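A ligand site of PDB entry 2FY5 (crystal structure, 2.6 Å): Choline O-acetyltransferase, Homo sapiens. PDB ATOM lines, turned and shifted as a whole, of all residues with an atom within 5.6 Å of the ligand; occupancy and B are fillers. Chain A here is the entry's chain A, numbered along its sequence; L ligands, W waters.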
ATOM      1  N   PRO A  98     -15.360  14.451  -1.059  1.00  0.00           N
ATOM      2  CA  PRO A  98     -15.527  13.056  -0.649  1.00  0.00           C
ATOM      3  C   PRO A  98     -16.684  12.392  -1.375  1.00  0.00           C
ATOM      4  O   PRO A  98     -17.530  13.063  -1.980  1.00  0.00           O
ATOM      5  CB  PRO A  98     -15.806  13.184   0.842  1.00  0.00           C
ATOM      6  CG  PRO A  98     -16.658  14.399   0.873  1.00  0.00           C
ATOM      7  CD  PRO A  98     -15.883  15.360  -0.022  1.00  0.00           C
ATOM      8  N   LYS A 142     -23.146  11.346  20.849  1.00  0.00           N
ATOM      9  CA  LYS A 142     -23.053   9.916  21.117  1.00  0.00           C
ATOM     10  C   LYS A 142     -21.565   9.639  21.205  1.00  0.00           C
ATOM     11  O   LYS A 142     -20.802  10.528  20.802  1.00  0.00           O
ATOM     12  CB  LYS A 142     -23.800   9.107  20.034  1.00  0.00           C
ATOM     13  CG  LYS A 142     -25.258   9.537  19.849  1.00  0.00           C
ATOM     14  CD  LYS A 142     -26.074   8.555  18.983  1.00  0.00           C
ATOM     15  CE  LYS A 142     -27.539   8.944  18.925  1.00  0.00           C
ATOM     16  NZ  LYS A 142     -28.311   8.028  18.038  1.00  0.00           N
ATOM     17  N   GLY A 143     -21.079   8.512  21.690  1.00  0.00           N
ATOM     18  CA  GLY A 143     -19.628   8.259  21.677  1.00  0.00           C
ATOM     19  C   GLY A 143     -18.815   8.908  22.827  1.00  0.00           C
ATOM     20  O   GLY A 143     -18.807   8.404  23.956  1.00  0.00           O
ATOM     21  N   GLN A 144     -18.144  10.016  22.551  1.00  0.00           N
ATOM     22  CA  GLN A 144     -17.331  10.696  23.549  1.00  0.00           C
ATOM     23  C   GLN A 144     -17.975  11.979  24.084  1.00  0.00           C
ATOM     24  O   GLN A 144     -17.819  13.062  23.493  1.00  0.00           O
ATOM     25  CB  GLN A 144     -15.942  10.957  22.980  1.00  0.00           C
ATOM     26  CG  GLN A 144     -15.072   9.713  22.854  1.00  0.00           C
ATOM     27  CD  GLN A 144     -14.254   9.489  24.098  1.00  0.00           C
ATOM     28  OE1 GLN A 144     -14.414  10.195  25.078  1.00  0.00           O
ATOM     29  NE2 GLN A 144     -13.386   8.522  24.100  1.00  0.00           N
ATOM     30  N   HIS A 324     -17.202  19.428  -0.124  1.00  0.00           N
ATOM     31  CA  HIS A 324     -16.902  19.573   1.287  1.00  0.00           C
ATOM     32  C   HIS A 324     -17.170  20.903   2.040  1.00  0.00           C
ATOM     33  O   HIS A 324     -17.694  20.875   3.157  1.00  0.00           O
ATOM     34  CB  HIS A 324     -15.448  19.181   1.498  1.00  0.00           C
ATOM     35  CG  HIS A 324     -15.203  18.371   2.736  1.00  0.00           C
ATOM     36  ND1 HIS A 324     -15.874  18.570   3.922  1.00  0.00           N
ATOM     37  CD2 HIS A 324     -14.344  17.343   2.967  1.00  0.00           C
ATOM     38  CE1 HIS A 324     -15.449  17.704   4.838  1.00  0.00           C
ATOM     39  NE2 HIS A 324     -14.520  16.945   4.276  1.00  0.00           N
ATOM     40  N   PHE A 327     -20.479  21.295   4.434  1.00  0.00           N
ATOM     41  CA  PHE A 327     -20.858  20.424   5.557  1.00  0.00           C
ATOM     42  C   PHE A 327     -19.916  19.251   5.611  1.00  0.00           C
ATOM     43  O   PHE A 327     -19.202  19.003   4.651  1.00  0.00           O
ATOM     44  CB  PHE A 327     -22.308  19.938   5.355  1.00  0.00           C
ATOM     45  CG  PHE A 327     -22.503  19.423   3.958  1.00  0.00           C
ATOM     46  CD1 PHE A 327     -22.001  18.167   3.622  1.00  0.00           C
ATOM     47  CD2 PHE A 327     -23.146  20.168   2.975  1.00  0.00           C
ATOM     48  CE1 PHE A 327     -22.118  17.668   2.323  1.00  0.00           C
ATOM     49  CE2 PHE A 327     -23.267  19.677   1.666  1.00  0.00           C
ATOM     50  CZ  PHE A 327     -22.753  18.429   1.332  1.00  0.00           C
ATOM     51  N   ASP A 328     -19.916  18.544   6.734  1.00  0.00           N
ATOM     52  CA  ASP A 328     -19.055  17.376   6.901  1.00  0.00           C
ATOM     53  C   ASP A 328     -19.771  16.021   6.809  1.00  0.00           C
ATOM     54  O   ASP A 328     -21.011  15.950   6.828  1.00  0.00           O
ATOM     55  CB  ASP A 328     -18.298  17.465   8.220  1.00  0.00           C
ATOM     56  CG  ASP A 328     -17.507  18.756   8.341  1.00  0.00           C
ATOM     57  OD1 ASP A 328     -16.776  19.091   7.371  1.00  0.00           O
ATOM     58  OD2 ASP A 328     -17.614  19.447   9.383  1.00  0.00           O
ATOM     59  N   GLY A 329     -18.974  14.955   6.696  1.00  0.00           N
ATOM     60  CA  GLY A 329     -19.469  13.582   6.536  1.00  0.00           C
ATOM     61  C   GLY A 329     -20.579  13.105   7.505  1.00  0.00           C
ATOM     62  O   GLY A 329     -21.520  12.431   7.061  1.00  0.00           O
ATOM     63  N   ILE A 330     -20.512  13.432   8.774  1.00  0.00           N
ATOM     64  CA  ILE A 330     -21.544  12.977   9.706  1.00  0.00           C
ATOM     65  C   ILE A 330     -22.937  13.429   9.260  1.00  0.00           C
ATOM     66  O   ILE A 330     -23.871  12.618   9.172  1.00  0.00           O
ATOM     67  CB  ILE A 330     -21.276  13.487  11.156  1.00  0.00           C
ATOM     68  CG1 ILE A 330     -19.885  13.042  11.638  1.00  0.00           C
ATOM     69  CG2 ILE A 330     -22.321  12.928  12.131  1.00  0.00           C
ATOM     70  CD1 ILE A 330     -19.706  11.539  11.662  1.00  0.00           C
ATOM     71  N   LYS A 400     -15.708  -3.208  17.165  1.00  0.00           N
ATOM     72  CA  LYS A 400     -15.924  -2.489  18.412  1.00  0.00           C
ATOM     73  C   LYS A 400     -16.092  -3.454  19.593  1.00  0.00           C
ATOM     74  O   LYS A 400     -15.374  -3.341  20.593  1.00  0.00           O
ATOM     75  CB  LYS A 400     -17.154  -1.574  18.292  1.00  0.00           C
ATOM     76  CG  LYS A 400     -16.997  -0.440  17.275  1.00  0.00           C
ATOM     77  CD  LYS A 400     -18.362   0.119  16.851  1.00  0.00           C
ATOM     78  CE  LYS A 400     -19.085   0.807  17.995  1.00  0.00           C
ATOM     79  NZ  LYS A 400     -20.524   1.047  17.682  1.00  0.00           N
ATOM     80  N   LYS A 404     -14.085  -2.941  22.962  1.00  0.00           N
ATOM     81  CA  LYS A 404     -14.732  -2.512  24.201  1.00  0.00           C
ATOM     82  C   LYS A 404     -14.420  -3.465  25.352  1.00  0.00           C
ATOM     83  O   LYS A 404     -14.354  -3.051  26.509  1.00  0.00           O
ATOM     84  CB  LYS A 404     -16.250  -2.440  24.036  1.00  0.00           C
ATOM     85  CG  LYS A 404     -16.743  -1.278  23.204  1.00  0.00           C
ATOM     86  CD  LYS A 404     -18.240  -1.325  23.103  1.00  0.00           C
ATOM     87  CE  LYS A 404     -18.774  -0.204  22.275  1.00  0.00           C
ATOM     88  NZ  LYS A 404     -20.242  -0.393  22.104  1.00  0.00           N
ATOM     89  N   LYS A 407     -11.539  -2.458  27.566  1.00  0.00           N
ATOM     90  CA  LYS A 407     -11.624  -1.203  28.299  1.00  0.00           C
ATOM     91  C   LYS A 407     -10.981  -0.095  27.445  1.00  0.00           C
ATOM     92  O   LYS A 407     -10.271   0.777  27.951  1.00  0.00           O
ATOM     93  CB  LYS A 407     -10.900  -1.312  29.648  1.00  0.00           C
ATOM     94  CG  LYS A 407     -11.577  -2.257  30.612  1.00  0.00           C
ATOM     95  CD  LYS A 407     -10.739  -2.424  31.868  1.00  0.00           C
ATOM     96  CE  LYS A 407     -11.491  -3.228  32.931  1.00  0.00           C
ATOM     97  NZ  LYS A 407     -10.648  -3.543  34.132  1.00  0.00           N
ATOM     98  N   CYS A 408     -11.245  -0.151  26.147  1.00  0.00           N
ATOM     99  CA  CYS A 408     -10.700   0.823  25.230  1.00  0.00           C
ATOM    100  C   CYS A 408     -11.757   1.495  24.353  1.00  0.00           C
ATOM    101  O   CYS A 408     -12.804   0.917  24.064  1.00  0.00           O
ATOM    102  CB  CYS A 408      -9.645   0.166  24.330  1.00  0.00           C
ATOM    103  SG  CYS A 408      -8.086  -0.222  25.167  1.00  0.00           S
ATOM    104  N   SER A 409     -11.462   2.724  23.958  1.00  0.00           N
ATOM    105  CA  SER A 409     -12.301   3.498  23.062  1.00  0.00           C
ATOM    106  C   SER A 409     -12.003   2.916  21.678  1.00  0.00           C
ATOM    107  O   SER A 409     -10.839   2.827  21.272  1.00  0.00           O
ATOM    108  CB  SER A 409     -11.937   4.993  23.140  1.00  0.00           C
ATOM    109  OG  SER A 409     -12.671   5.753  22.183  1.00  0.00           O
ATOM    110  N   PRO A 410     -13.037   2.451  20.952  1.00  0.00           N
ATOM    111  CA  PRO A 410     -12.795   1.873  19.628  1.00  0.00           C
ATOM    112  C   PRO A 410     -12.003   2.833  18.744  1.00  0.00           C
ATOM    113  O   PRO A 410     -10.993   2.446  18.135  1.00  0.00           O
ATOM    114  CB  PRO A 410     -14.195   1.610  19.100  1.00  0.00           C
ATOM    115  CG  PRO A 410     -14.919   1.208  20.328  1.00  0.00           C
ATOM    116  CD  PRO A 410     -14.438   2.227  21.370  1.00  0.00           C
ATOM    117  N   ASP A 411     -12.442   4.081  18.684  1.00  0.00           N
ATOM    118  CA  ASP A 411     -11.776   5.062  17.857  1.00  0.00           C
ATOM    119  C   ASP A 411     -10.336   5.314  18.277  1.00  0.00           C
ATOM    120  O   ASP A 411      -9.476   5.549  17.428  1.00  0.00           O
ATOM    121  CB  ASP A 411     -12.543   6.387  17.847  1.00  0.00           C
ATOM    122  CG  ASP A 411     -12.017   7.342  16.801  1.00  0.00           C
ATOM    123  OD1 ASP A 411     -12.203   7.049  15.597  1.00  0.00           O
ATOM    124  OD2 ASP A 411     -11.420   8.371  17.168  1.00  0.00           O
ATOM    125  N   ALA A 412     -10.073   5.298  19.571  1.00  0.00           N
ATOM    126  CA  ALA A 412      -8.713   5.517  20.048  1.00  0.00           C
ATOM    127  C   ALA A 412      -7.865   4.319  19.614  1.00  0.00           C
ATOM    128  O   ALA A 412      -6.737   4.487  19.142  1.00  0.00           O
ATOM    129  CB  ALA A 412      -8.700   5.630  21.562  1.00  0.00           C
ATOM    130  N   GLU A 434      -6.976  14.067  12.512  1.00  0.00           N
ATOM    131  CA  GLU A 434      -8.195  13.283  12.769  1.00  0.00           C
ATOM    132  C   GLU A 434      -9.324  14.250  13.078  1.00  0.00           C
ATOM    133  O   GLU A 434      -9.268  15.023  14.037  1.00  0.00           O
ATOM    134  CB  GLU A 434      -8.072  12.321  13.958  1.00  0.00           C
ATOM    135  CG  GLU A 434      -9.375  11.490  14.122  1.00  0.00           C
ATOM    136  CD  GLU A 434      -9.451  10.638  15.392  1.00  0.00           C
ATOM    137  OE1 GLU A 434      -8.440  10.507  16.119  1.00  0.00           O
ATOM    138  OE2 GLU A 434     -10.546  10.090  15.650  1.00  0.00           O
ATOM    139  N   SER A 435     -10.358  14.197  12.248  1.00  0.00           N
ATOM    140  CA  SER A 435     -11.535  15.042  12.390  1.00  0.00           C
ATOM    141  C   SER A 435     -12.240  14.833  13.710  1.00  0.00           C
ATOM    142  O   SER A 435     -12.750  13.754  13.988  1.00  0.00           O
ATOM    143  CB  SER A 435     -12.541  14.744  11.280  1.00  0.00           C
ATOM    144  OG  SER A 435     -11.962  14.923  10.012  1.00  0.00           O
ATOM    145  N   ALA A 436     -12.273  15.885  14.508  1.00  0.00           N
ATOM    146  CA  ALA A 436     -12.945  15.877  15.782  1.00  0.00           C
ATOM    147  C   ALA A 436     -14.117  16.813  15.583  1.00  0.00           C
ATOM    148  O   ALA A 436     -13.925  17.980  15.239  1.00  0.00           O
ATOM    149  CB  ALA A 436     -12.019  16.412  16.868  1.00  0.00           C
ATOM    150  N   SER A 437     -15.334  16.322  15.758  1.00  0.00           N
ATOM    151  CA  SER A 437     -16.479  17.179  15.567  1.00  0.00           C
ATOM    152  C   SER A 437     -16.713  18.073  16.768  1.00  0.00           C
ATOM    153  O   SER A 437     -16.712  17.601  17.909  1.00  0.00           O
ATOM    154  CB  SER A 437     -17.748  16.348  15.326  1.00  0.00           C
ATOM    155  OG  SER A 437     -18.902  17.179  15.436  1.00  0.00           O
ATOM    156  N   VAL A 446     -15.287  21.341  12.830  1.00  0.00           N
ATOM    157  CA  VAL A 446     -14.345  20.364  13.378  1.00  0.00           C
ATOM    158  C   VAL A 446     -13.026  21.005  13.758  1.00  0.00           C
ATOM    159  O   VAL A 446     -12.624  21.995  13.162  1.00  0.00           O
ATOM    160  CB  VAL A 446     -13.966  19.259  12.353  1.00  0.00           C
ATOM    161  CG1 VAL A 446     -15.208  18.511  11.893  1.00  0.00           C
ATOM    162  CG2 VAL A 446     -13.249  19.876  11.169  1.00  0.00           C
ATOM    163  N   ILE A 449      -7.474  16.492  16.033  1.00  0.00           N
ATOM    164  CA  ILE A 449      -6.948  15.605  17.063  1.00  0.00           C
ATOM    165  C   ILE A 449      -5.603  15.123  16.495  1.00  0.00           C
ATOM    166  O   ILE A 449      -5.589  14.451  15.462  1.00  0.00           O
ATOM    167  CB  ILE A 449      -7.840  14.367  17.276  1.00  0.00           C
ATOM    168  CG1 ILE A 449      -9.200  14.786  17.826  1.00  0.00           C
ATOM    169  CG2 ILE A 449      -7.161  13.390  18.206  1.00  0.00           C
ATOM    170  CD1 ILE A 449     -10.190  13.653  17.977  1.00  0.00           C
ATOM    171  N   THR A 490      -8.565  13.358  22.375  1.00  0.00           N
ATOM    172  CA  THR A 490      -9.882  13.392  21.774  1.00  0.00           C
ATOM    173  C   THR A 490     -10.809  14.233  22.647  1.00  0.00           C
ATOM    174  O   THR A 490     -11.394  15.224  22.186  1.00  0.00           O
ATOM    175  CB  THR A 490     -10.434  11.962  21.620  1.00  0.00           C
ATOM    176  OG1 THR A 490      -9.648  11.260  20.644  1.00  0.00           O
ATOM    177  CG2 THR A 490     -11.878  12.000  21.160  1.00  0.00           C
ATOM    178  N   ILE A 494     -12.732  17.626  21.155  1.00  0.00           N
ATOM    179  CA  ILE A 494     -14.166  17.809  21.019  1.00  0.00           C
ATOM    180  C   ILE A 494     -14.798  18.776  22.008  1.00  0.00           C
ATOM    181  O   ILE A 494     -15.985  19.087  21.882  1.00  0.00           O
ATOM    182  CB  ILE A 494     -14.921  16.486  21.104  1.00  0.00           C
ATOM    183  CG1 ILE A 494     -14.738  15.872  22.494  1.00  0.00           C
ATOM    184  CG2 ILE A 494     -14.449  15.548  20.013  1.00  0.00           C
ATOM    185  CD1 ILE A 494     -15.511  14.589  22.693  1.00  0.00           C
ATOM    186  N   SER A 537     -10.221  10.140   9.504  1.00  0.00           N
ATOM    187  CA  SER A 537     -11.524  10.537  10.008  1.00  0.00           C
ATOM    188  C   SER A 537     -12.406   9.302  10.140  1.00  0.00           C
ATOM    189  O   SER A 537     -12.154   8.274   9.501  1.00  0.00           O
ATOM    190  CB  SER A 537     -12.201  11.536   9.077  1.00  0.00           C
ATOM    191  OG  SER A 537     -12.929  10.874   8.065  1.00  0.00           O
ATOM    192  N   GLN A 538     -13.429   9.398  10.967  1.00  0.00           N
ATOM    193  CA  GLN A 538     -14.357   8.296  11.137  1.00  0.00           C
ATOM    194  C   GLN A 538     -15.717   8.728  10.628  1.00  0.00           C
ATOM    195  O   GLN A 538     -16.192   9.809  10.946  1.00  0.00           O
ATOM    196  CB  GLN A 538     -14.476   7.906  12.606  1.00  0.00           C
ATOM    197  CG  GLN A 538     -15.508   6.805  12.835  1.00  0.00           C
ATOM    198  CD  GLN A 538     -15.843   6.643  14.297  1.00  0.00           C
ATOM    199  OE1 GLN A 538     -16.999   6.821  14.698  1.00  0.00           O
ATOM    200  NE2 GLN A 538     -14.845   6.298  15.110  1.00  0.00           N
ATOM    201  N   VAL A 539     -16.336   7.873   9.825  1.00  0.00           N
ATOM    202  CA  VAL A 539     -17.669   8.130   9.298  1.00  0.00           C
ATOM    203  C   VAL A 539     -18.389   6.803   9.453  1.00  0.00           C
ATOM    204  O   VAL A 539     -18.376   5.965   8.563  1.00  0.00           O
ATOM    205  CB  VAL A 539     -17.657   8.540   7.827  1.00  0.00           C
ATOM    206  CG1 VAL A 539     -19.057   8.926   7.385  1.00  0.00           C
ATOM    207  CG2 VAL A 539     -16.699   9.685   7.600  1.00  0.00           C
ATOM    208  N   CYS A 547     -17.881   5.984   3.172  1.00  0.00           N
ATOM    209  CA  CYS A 547     -17.318   7.260   2.735  1.00  0.00           C
ATOM    210  C   CYS A 547     -15.835   7.160   2.381  1.00  0.00           C
ATOM    211  O   CYS A 547     -15.140   6.267   2.869  1.00  0.00           O
ATOM    212  CB  CYS A 547     -17.532   8.282   3.850  1.00  0.00           C
ATOM    213  SG  CYS A 547     -17.117   9.980   3.445  1.00  0.00           S
ATOM    214  N   TYR A 549     -12.139   9.531   0.530  1.00  0.00           N
ATOM    215  CA  TYR A 549     -11.536  10.747  -0.020  1.00  0.00           C
ATOM    216  C   TYR A 549     -10.026  10.629  -0.241  1.00  0.00           C
ATOM    217  O   TYR A 549      -9.378   9.741   0.312  1.00  0.00           O
ATOM    218  CB  TYR A 549     -11.862  11.938   0.888  1.00  0.00           C
ATOM    219  CG  TYR A 549     -11.487  11.763   2.339  1.00  0.00           C
ATOM    220  CD1 TYR A 549     -10.241  12.160   2.816  1.00  0.00           C
ATOM    221  CD2 TYR A 549     -12.410  11.227   3.250  1.00  0.00           C
ATOM    222  CE1 TYR A 549      -9.901  12.028   4.182  1.00  0.00           C
ATOM    223  CE2 TYR A 549     -12.089  11.088   4.608  1.00  0.00           C
ATOM    224  CZ  TYR A 549     -10.839  11.497   5.064  1.00  0.00           C
ATOM    225  OH  TYR A 549     -10.539  11.417   6.405  1.00  0.00           O
ATOM    226  N   CYS A 560     -10.364   6.756   5.819  1.00  0.00           N
ATOM    227  CA  CYS A 560     -11.699   6.939   6.367  1.00  0.00           C
ATOM    228  C   CYS A 560     -12.204   5.570   6.786  1.00  0.00           C
ATOM    229  O   CYS A 560     -12.276   4.650   5.973  1.00  0.00           O
ATOM    230  CB  CYS A 560     -12.623   7.592   5.322  1.00  0.00           C
ATOM    231  SG  CYS A 560     -14.242   8.139   5.985  1.00  0.00           S
ATOM    232  N   TYR A 561     -12.544   5.420   8.050  1.00  0.00           N
ATOM    233  CA  TYR A 561     -13.025   4.129   8.526  1.00  0.00           C
ATOM    234  C   TYR A 561     -14.417   4.141   9.139  1.00  0.00           C
ATOM    235  O   TYR A 561     -14.903   5.166   9.622  1.00  0.00           O
ATOM    236  CB  TYR A 561     -12.035   3.540   9.537  1.00  0.00           C
ATOM    237  CG  TYR A 561     -11.649   4.495  10.635  1.00  0.00           C
ATOM    238  CD1 TYR A 561     -10.642   5.434  10.444  1.00  0.00           C
ATOM    239  CD2 TYR A 561     -12.325   4.507  11.848  1.00  0.00           C
ATOM    240  CE1 TYR A 561     -10.315   6.352  11.417  1.00  0.00           C
ATOM    241  CE2 TYR A 561     -12.015   5.418  12.843  1.00  0.00           C
ATOM    242  CZ  TYR A 561     -11.010   6.342  12.619  1.00  0.00           C
ATOM    243  OH  TYR A 561     -10.708   7.275  13.578  1.00  0.00           O
HETATM  244  N1  LIG L   1     -12.875   2.715  27.902  1.00  0.00           N
HETATM  245  C1  LIG L   1     -13.972   2.213  27.363  1.00  0.00           C
HETATM  246  N2  LIG L   1     -14.435   0.992  27.753  1.00  0.00           N
HETATM  247  C2  LIG L   1     -15.542   0.451  27.224  1.00  0.00           C
HETATM  248  N3  LIG L   1     -16.233   1.134  26.269  1.00  0.00           N
HETATM  249  C3  LIG L   1     -15.821   2.354  25.831  1.00  0.00           C
HETATM  250  C4  LIG L   1     -14.669   2.923  26.384  1.00  0.00           C
HETATM  251  N4  LIG L   1     -14.471   4.093  25.811  1.00  0.00           N
HETATM  252  C5  LIG L   1     -15.466   4.272  24.929  1.00  0.00           C
HETATM  253  N5  LIG L   1     -16.293   3.235  24.930  1.00  0.00           N
HETATM  254  C6  LIG L   1     -17.508   3.063  24.069  1.00  0.00           C
HETATM  255  O1  LIG L   1     -17.197   3.009  22.657  1.00  0.00           O
HETATM  256  C7  LIG L   1     -18.563   4.188  24.133  1.00  0.00           C
HETATM  257  O2  LIG L   1     -19.333   4.100  25.331  1.00  0.00           O
HETATM  258  C8  LIG L   1     -19.374   3.884  22.888  1.00  0.00           C
HETATM  259  O3  LIG L   1     -20.337   2.848  23.113  1.00  0.00           O
HETATM  260  P1  LIG L   1     -21.584   2.702  22.110  1.00  0.00           P
HETATM  261  O4  LIG L   1     -21.083   1.866  20.816  1.00  0.00           O
HETATM  262  O5  LIG L   1     -22.668   1.821  22.907  1.00  0.00           O
HETATM  263  O6  LIG L   1     -22.115   4.049  21.739  1.00  0.00           O
HETATM  264  C9  LIG L   1     -18.317   3.490  21.871  1.00  0.00           C
HETATM  265  C10 LIG L   1     -17.905   4.743  21.092  1.00  0.00           C
HETATM  266  O7  LIG L   1     -16.579   4.561  20.609  1.00  0.00           O
HETATM  267  P2  LIG L   1     -15.508   5.750  20.640  1.00  0.00           P
HETATM  268  O8  LIG L   1     -14.187   5.119  20.401  1.00  0.00           O
HETATM  269  O9  LIG L   1     -15.631   6.479  21.914  1.00  0.00           O
HETATM  270  O10 LIG L   1     -15.943   6.599  19.343  1.00  0.00           O
HETATM  271  P3  LIG L   1     -16.630   8.036  19.385  1.00  0.00           P
HETATM  272  O11 LIG L   1     -16.497   8.673  20.689  1.00  0.00           O
HETATM  273  O12 LIG L   1     -18.007   7.782  18.895  1.00  0.00           O
HETATM  274  O13 LIG L   1     -15.775   8.830  18.315  1.00  0.00           O
HETATM  275  C11 LIG L   1     -14.687   9.683  18.690  1.00  0.00           C
HETATM  276  C12 LIG L   1     -14.636  10.852  17.703  1.00  0.00           C
HETATM  277  C13 LIG L   1     -14.387  10.272  16.284  1.00  0.00           C
HETATM  278  C14 LIG L   1     -13.473  11.783  18.083  1.00  0.00           C
HETATM  279  C15 LIG L   1     -16.010  11.565  17.800  1.00  0.00           C
HETATM  280  O14 LIG L   1     -16.151  12.276  19.046  1.00  0.00           O
HETATM  281  C16 LIG L   1     -16.255  12.557  16.664  1.00  0.00           C
HETATM  282  O15 LIG L   1     -15.979  13.769  16.771  1.00  0.00           O
HETATM  283  N6  LIG L   1     -16.782  11.955  15.583  1.00  0.00           N
HETATM  284  C17 LIG L   1     -17.102  12.684  14.357  1.00  0.00           C
HETATM  285  C18 LIG L   1     -15.964  12.477  13.378  1.00  0.00           C
HETATM  286  C19 LIG L   1     -16.235  13.270  12.107  1.00  0.00           C
HETATM  287  O16 LIG L   1     -16.292  14.513  12.166  1.00  0.00           O
HETATM  288  N7  LIG L   1     -16.392  12.565  10.984  1.00  0.00           N
HETATM  289  C20 LIG L   1     -16.654  13.215   9.671  1.00  0.00           C
HETATM  290  C21 LIG L   1     -15.396  14.015   9.241  1.00  0.00           C
HETATM  291  S1  LIG L   1     -15.592  14.877   7.666  1.00  0.00           S
HETATM  292  C22 LIG L   1     -15.033  13.848   6.345  1.00  0.00           C
HETATM  293  C23 LIG L   1     -16.016  13.403   5.294  1.00  0.00           C
HETATM  294  O17 LIG L   1     -16.528  12.307   5.367  1.00  0.00           O
HETATM  295  C24 LIG L   1     -16.220  14.458   4.223  1.00  0.00           C
HETATM  296  O   HOH W   1     -18.013   9.164  15.524  1.00  0.00           O
HETATM  297  O   HOH W   2     -18.945  16.002  12.131  1.00  0.00           O
HETATM  298  O   HOH W   3     -17.583  14.919  19.071  1.00  0.00           O
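OG of Ser 409 is in hydrogen-bond range of O8 of the ligand, at 2.4 Å. O8 of the ligand sits at hydrogen-bond distance from N of Asp 411 (2.7 Å). The side-chain amino group (NZ) of Lys 404 is in salt-bridge range of an oxygen (O4) of the ligand (2.7 Å). A nitrogen (N7) of the ligand lies within hydrogen-bond range of the backbone carbonyl oxygen (O) of Gln 538, 2.8 Å away. N of Gln 144 sits close to O11 of the ligand, 2.8 Å away. An oxygen (O15) of the ligand lies within hydrogen-bond range of the backbone NH of Ser 437. An oxygen (O17) of the ligand sits at hydrogen-bond distance from the side-chain sulfur (SG) of Cys 547, 3.1 Å away. The backbone carbonyl oxygen of Lys 407 sits at hydrogen-bond distance from a nitrogen (N1) of the ligand (3.2 Å). The side-chain amino group (NZ) of Lys 400 is in salt-bridge range of an oxygen (O4) of the ligand, 3.3 Å away. A sulfur (S1) of the ligand lies close to the backbone NH of Gly 329 (3.5 Å).
The side-chain hydroxyl (OG) of Ser 409 sits at hydrogen-bond distance from the side-chain amide nitrogen (NE2) of Gln 144, 3.4 Å away. NE2 of Gln 538 is in hydrogen-bond range of OD1 of Asp 411, at 2.8 Å. The side-chain carboxylate (OE2) of Glu 434 lies close to the side-chain carboxylate (OD2) of Asp 411, at 2.5 Å. OD1 of Asp 411 is in hydrogen-bond range of OH of Tyr 561, 2.5 Å away. The backbone carbonyl oxygen of Phe 327 is in hydrogen-bond range of a ring nitrogen (ND1) of His 324 (3.4 Å). The side-chain sulfur of Cys 560 lies within hydrogen-bond range of the backbone carbonyl oxygen of Cys 547, at 3.7 Å. The backbone NH of Ile 449 is in hydrogen-bond range of the backbone carbonyl oxygen of Glu 434. The side-chain carboxylate (OE2) of Glu 434 sits at hydrogen-bond distance from the side-chain hydroxyl (OH) of Tyr 561, at 3.5 Å.
The backbone nitrogen (N) of Pro 410 sits close to an oxygen (O8) of the ligand (3.0 Å). Merely in contact with the ligand: His 324, Gly 143, Pro 98, Val 539, Thr 490, Ser 435, Ile 330, Cys 408, Ala 436, Ile 449, Asp 328, Ile 494 and Glu 434. Hydrophobic or aromatic side chains within 4 Å of the ligand: Pro 98, His 324, Ile 330, Pro 410, Ile 449, Ile 494 and Val 539. Within 4 Å of the ligand: Pro 98, Gly 143, Gln 144, His 324, Asp 328, Gly 329, Ile 330, Lys 400, Lys 404, Lys 407, Cys 408, Ser 409, Pro 410, Asp 411, Glu 434, Ser 435, Ala 436, Ser 437, Ile 449, Thr 490, Ile 494, Gln 538, Val 539 and Cys 547. The nearest printed residue that does not touch the ligand is Ser 537 (4.03 Å).
Water W3 bridges an oxygen (O14) of the ligand (3.0 Å) and the backbone carbonyl oxygen (O) of Ser 437 (3.0 Å). Water W1 bridges OE1 of Gln 538 and N6 of the ligand.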
